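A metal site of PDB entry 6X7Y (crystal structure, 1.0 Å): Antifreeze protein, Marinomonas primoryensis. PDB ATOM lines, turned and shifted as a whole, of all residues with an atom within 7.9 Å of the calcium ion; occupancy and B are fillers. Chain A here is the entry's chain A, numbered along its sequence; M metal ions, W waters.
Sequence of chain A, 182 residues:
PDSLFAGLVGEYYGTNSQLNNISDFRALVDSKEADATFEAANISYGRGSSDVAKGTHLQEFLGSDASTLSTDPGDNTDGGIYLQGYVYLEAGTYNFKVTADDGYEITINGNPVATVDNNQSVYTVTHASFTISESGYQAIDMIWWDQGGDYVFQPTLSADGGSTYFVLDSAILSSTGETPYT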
ATOM      1  N   THR A  15     -33.696  14.206  17.476  1.00  0.00           N
ATOM      2  CA  THR A  15     -33.127  13.153  18.343  1.00  0.00           C
ATOM      3  C   THR A  15     -33.434  13.523  19.799  1.00  0.00           C
ATOM      4  O   THR A  15     -33.622  14.678  20.133  1.00  0.00           O
ATOM      5  CB  THR A  15     -31.607  13.011  18.096  1.00  0.00           C
ATOM      6  OG1 THR A  15     -31.073  11.954  18.900  1.00  0.00           O
ATOM      7  CG2 THR A  15     -30.803  14.249  18.444  1.00  0.00           C
ATOM      8  N   ASN A  16     -33.399  12.501  20.670  1.00  0.00           N
ATOM      9  CA  ASN A  16     -33.474  12.713  22.106  1.00  0.00           C
ATOM     10  C   ASN A  16     -32.116  12.514  22.780  1.00  0.00           C
ATOM     11  O   ASN A  16     -32.031  12.487  24.035  1.00  0.00           O
ATOM     12  CB  ASN A  16     -34.567  11.853  22.727  1.00  0.00           C
ATOM     13  CG  ASN A  16     -35.902  12.120  22.080  1.00  0.00           C
ATOM     14  OD1 ASN A  16     -36.299  13.316  21.882  1.00  0.00           O
ATOM     15  ND2 ASN A  16     -36.631  11.100  21.790  1.00  0.00           N
ATOM     16  N   SER A  17     -31.053  12.428  21.993  1.00  0.00           N
ATOM     17  CA  SER A  17     -29.695  12.492  22.443  1.00  0.00           C
ATOM     18  C   SER A  17     -29.167  13.939  22.334  1.00  0.00           C
ATOM     19  O   SER A  17     -29.763  14.761  21.647  1.00  0.00           O
ATOM     20  CB  SER A  17     -28.811  11.571  21.611  1.00  0.00           C
ATOM     21  OG  SER A  17     -28.633  12.037  20.266  1.00  0.00           O
ATOM     22  N   GLN A  18     -28.073  14.212  23.039  1.00  0.00           N
ATOM     23  CA  GLN A  18     -27.491  15.554  23.006  1.00  0.00           C
ATOM     24  C   GLN A  18     -26.662  15.744  21.756  1.00  0.00           C
ATOM     25  O   GLN A  18     -25.761  14.948  21.446  1.00  0.00           O
ATOM     26  CB  GLN A  18     -26.640  15.769  24.244  1.00  0.00           C
ATOM     27  CG  GLN A  18     -25.747  17.032  24.237  1.00  0.00           C
ATOM     28  CD  GLN A  18     -26.510  18.334  24.297  1.00  0.00           C
ATOM     29  OE1 GLN A  18     -27.723  18.383  24.134  1.00  0.00           O
ATOM     30  NE2 GLN A  18     -25.790  19.423  24.476  1.00  0.00           N
ATOM     31  N   LEU A  19     -26.861  16.894  21.082  1.00  0.00           N
ATOM     32  CA  LEU A  19     -26.004  17.339  20.007  1.00  0.00           C
ATOM     33  C   LEU A  19     -25.013  18.361  20.551  1.00  0.00           C
ATOM     34  O   LEU A  19     -25.417  19.442  20.967  1.00  0.00           O
ATOM     35  CB  LEU A  19     -26.842  17.949  18.880  1.00  0.00           C
ATOM     36  CG  LEU A  19     -27.842  16.980  18.213  1.00  0.00           C
ATOM     37  CD1 LEU A  19     -28.724  17.732  17.245  1.00  0.00           C
ATOM     38  CD2 LEU A  19     -27.107  15.838  17.512  1.00  0.00           C
ATOM     39  N   ASN A  20     -23.723  18.006  20.574  1.00  0.00           N
ATOM     40  CA  ASN A  20     -22.698  18.903  21.103  1.00  0.00           C
ATOM     41  C   ASN A  20     -21.823  19.544  20.016  1.00  0.00           C
ATOM     42  O   ASN A  20     -21.106  20.504  20.304  1.00  0.00           O
ATOM     43  CB  ASN A  20     -21.762  18.158  22.044  1.00  0.00           C
ATOM     44  CG  ASN A  20     -22.380  17.916  23.401  1.00  0.00           C
ATOM     45  OD1 ASN A  20     -22.934  18.857  24.006  1.00  0.00           O
ATOM     46  ND2 ASN A  20     -22.262  16.720  23.884  1.00  0.00           N
ATOM     47  N   ASP A  51     -36.965  25.179  22.146  1.00  0.00           N
ATOM     48  CA  ASP A  51     -36.445  23.969  21.451  1.00  0.00           C
ATOM     49  C   ASP A  51     -37.002  23.837  20.036  1.00  0.00           C
ATOM     50  O   ASP A  51     -38.208  23.714  19.819  1.00  0.00           O
ATOM     51  CB  ASP A  51     -36.775  22.676  22.198  1.00  0.00           C
ATOM     52  CG  ASP A  51     -36.407  22.659  23.663  1.00  0.00           C
ATOM     53  OD1 ASP A  51     -35.379  23.206  24.043  1.00  0.00           O
ATOM     54  OD2 ASP A  51     -37.100  21.969  24.394  1.00  0.00           O
ATOM     55  N   THR A  77     -35.959  16.312  21.687  1.00  0.00           N
ATOM     56  CA  THR A  77     -35.292  17.334  22.481  1.00  0.00           C
ATOM     57  C   THR A  77     -34.349  18.214  21.644  1.00  0.00           C
ATOM     58  O   THR A  77     -34.206  19.405  21.932  1.00  0.00           O
ATOM     59  CB  THR A  77     -34.540  16.726  23.674  1.00  0.00           C
ATOM     60  OG1 THR A  77     -33.438  15.909  23.226  1.00  0.00           O
ATOM     61  CG2 THR A  77     -35.424  15.860  24.559  1.00  0.00           C
ATOM     62  N   ASP A  78     -33.698  17.614  20.659  1.00  0.00           N
ATOM     63  CA  ASP A  78     -32.652  18.202  19.884  1.00  0.00           C
ATOM     64  C   ASP A  78     -32.956  17.989  18.394  1.00  0.00           C
ATOM     65  O   ASP A  78     -33.637  17.020  18.035  1.00  0.00           O
ATOM     66  CB  ASP A  78     -31.280  17.555  20.205  1.00  0.00           C
ATOM     67  CG  ASP A  78     -30.746  17.800  21.601  1.00  0.00           C
ATOM     68  OD1 ASP A  78     -31.513  17.619  22.585  1.00  0.00           O
ATOM     69  OD2 ASP A  78     -29.552  18.187  21.744  1.00  0.00           O
ATOM     70  N   GLY A  79     -32.467  18.858  17.517  1.00  0.00           N
ATOM     71  CA  GLY A  79     -32.718  18.619  16.098  1.00  0.00           C
ATOM     72  C   GLY A  79     -31.914  19.560  15.262  1.00  0.00           C
ATOM     73  O   GLY A  79     -31.340  20.531  15.735  1.00  0.00           O
ATOM     74  N   ASP A 102     -27.659  26.732  17.458  1.00  0.00           N
ATOM     75  CA  ASP A 102     -26.351  26.458  18.032  1.00  0.00           C
ATOM     76  C   ASP A 102     -25.288  26.568  16.909  1.00  0.00           C
ATOM     77  O   ASP A 102     -25.088  27.670  16.389  1.00  0.00           O
ATOM     78  CB  ASP A 102     -26.387  25.116  18.797  1.00  0.00           C
ATOM     79  CG  ASP A 102     -27.087  25.295  20.119  1.00  0.00           C
ATOM     80  OD1 ASP A 102     -26.420  25.785  21.064  1.00  0.00           O
ATOM     81  OD2 ASP A 102     -28.306  24.978  20.219  1.00  0.00           O
ATOM     82  N   ASN A 119     -21.829  24.222  20.637  1.00  0.00           N
ATOM     83  CA  ASN A 119     -23.057  24.874  21.003  1.00  0.00           C
ATOM     84  C   ASN A 119     -22.777  26.322  21.399  1.00  0.00           C
ATOM     85  O   ASN A 119     -21.669  26.657  21.798  1.00  0.00           O
ATOM     86  CB  ASN A 119     -23.732  24.093  22.113  1.00  0.00           C
ATOM     87  CG  ASN A 119     -24.299  22.787  21.590  1.00  0.00           C
ATOM     88  OD1 ASN A 119     -24.729  22.720  20.459  1.00  0.00           O
ATOM     89  ND2 ASN A 119     -24.340  21.784  22.452  1.00  0.00           N
ATOM     90  N   TRP A 145     -27.695  22.928  13.852  1.00  0.00           N
ATOM     91  CA  TRP A 145     -28.531  22.228  14.816  1.00  0.00           C
ATOM     92  C   TRP A 145     -28.818  23.126  16.007  1.00  0.00           C
ATOM     93  O   TRP A 145     -28.163  24.133  16.246  1.00  0.00           O
ATOM     94  CB  TRP A 145     -27.868  20.903  15.261  1.00  0.00           C
ATOM     95  CG  TRP A 145     -26.708  21.107  16.194  1.00  0.00           C
ATOM     96  CD1 TRP A 145     -26.775  21.156  17.565  1.00  0.00           C
ATOM     97  CD2 TRP A 145     -25.340  21.405  15.851  1.00  0.00           C
ATOM     98  NE1 TRP A 145     -25.557  21.463  18.106  1.00  0.00           N
ATOM     99  CE2 TRP A 145     -24.673  21.643  17.090  1.00  0.00           C
ATOM    100  CE3 TRP A 145     -24.639  21.498  14.648  1.00  0.00           C
ATOM    101  CZ2 TRP A 145     -23.309  21.995  17.113  1.00  0.00           C
ATOM    102  CZ3 TRP A 145     -23.313  21.857  14.696  1.00  0.00           C
ATOM    103  CH2 TRP A 145     -22.670  22.105  15.903  1.00  0.00           C
ATOM    104  N   ASP A 146     -29.804  22.628  16.762  1.00  0.00           N
ATOM    105  CA  ASP A 146     -30.208  23.157  18.068  1.00  0.00           C
ATOM    106  C   ASP A 146     -30.103  22.019  19.097  1.00  0.00           C
ATOM    107  O   ASP A 146     -30.745  20.992  18.969  1.00  0.00           O
ATOM    108  CB  ASP A 146     -31.656  23.648  18.026  1.00  0.00           C
ATOM    109  CG  ASP A 146     -32.170  24.118  19.376  1.00  0.00           C
ATOM    110  OD1 ASP A 146     -31.333  24.710  20.116  1.00  0.00           O
ATOM    111  OD2 ASP A 146     -33.347  23.863  19.697  1.00  0.00           O
ATOM    112  N   GLN A 147     -29.300  22.287  20.126  1.00  0.00           N
ATOM    113  CA  GLN A 147     -29.193  21.351  21.286  1.00  0.00           C
ATOM    114  C   GLN A 147     -30.320  21.572  22.276  1.00  0.00           C
ATOM    115  O   GLN A 147     -30.429  20.785  23.248  1.00  0.00           O
ATOM    116  CB  GLN A 147     -27.836  21.513  21.976  1.00  0.00           C
ATOM    117  CG  GLN A 147     -27.671  22.830  22.751  1.00  0.00           C
ATOM    118  CD  GLN A 147     -28.052  22.726  24.192  1.00  0.00           C
ATOM    119  OE1 GLN A 147     -27.590  21.812  24.920  1.00  0.00           O
ATOM    120  NE2 GLN A 147     -28.876  23.651  24.664  1.00  0.00           N
ATOM    121  N   GLY A 148     -31.106  22.619  22.109  1.00  0.00           N
ATOM    122  CA  GLY A 148     -32.140  23.014  23.049  1.00  0.00           C
ATOM    123  C   GLY A 148     -32.141  24.501  23.254  1.00  0.00           C
ATOM    124  O   GLY A 148     -31.125  25.194  23.028  1.00  0.00           O
ATOM    125  N   GLY A 149     -33.283  25.018  23.705  1.00  0.00           N
ATOM    126  CA  GLY A 149     -33.413  26.418  24.025  1.00  0.00           C
ATOM    127  C   GLY A 149     -33.792  27.263  22.818  1.00  0.00           C
ATOM    128  O   GLY A 149     -34.766  26.976  22.117  1.00  0.00           O
HETATM  129 CA    CA M   1     -30.025  18.688  24.170  1.00  0.00          CA
HETATM  130  O   HOH W   1     -32.011  19.005  25.461  1.00  0.00           O
HETATM  131  O   HOH W   2     -29.293  20.011  26.075  1.00  0.00           O
HETATM  132  O   HOH W   3     -29.869  16.642  25.322  1.00  0.00           O
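The side-chain amide nitrogen of Gln 18 sits close to the side-chain amide nitrogen of Asn 119.
The side-chain amide nitrogen (NE2) of Gln 18 is in hydrogen-bond range of the side-chain amide oxygen (OD1) of Asn 20.
The side-chain carboxylate (OD2) of Asp 102 sits close to the backbone NH (N) of Gln 147, 2.9 Å away.
OD1 of Asp 78 sits close to OG1 of Thr 77 (2.7 Å).
The side-chain carboxylate (OD2) of Asp 78 lies close to the backbone NH (N) of Leu 19.
The backbone carbonyl oxygen (O) of Asp 78 lies within hydrogen-bond range of the backbone NH (N) of Thr 15.
The calcium ion is bound by OE1 of Gln 18 (2.3 Å), O of Gln 147 (2.3 Å), water W3 (2.4 Å), water W1 (2.4 Å), OD1 of Asp 78 (2.4 Å), water W2 (2.4 Å) and OD2 of Asp 78 (2.5 Å).
The calcium ion has seven donor atoms within binding distance.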
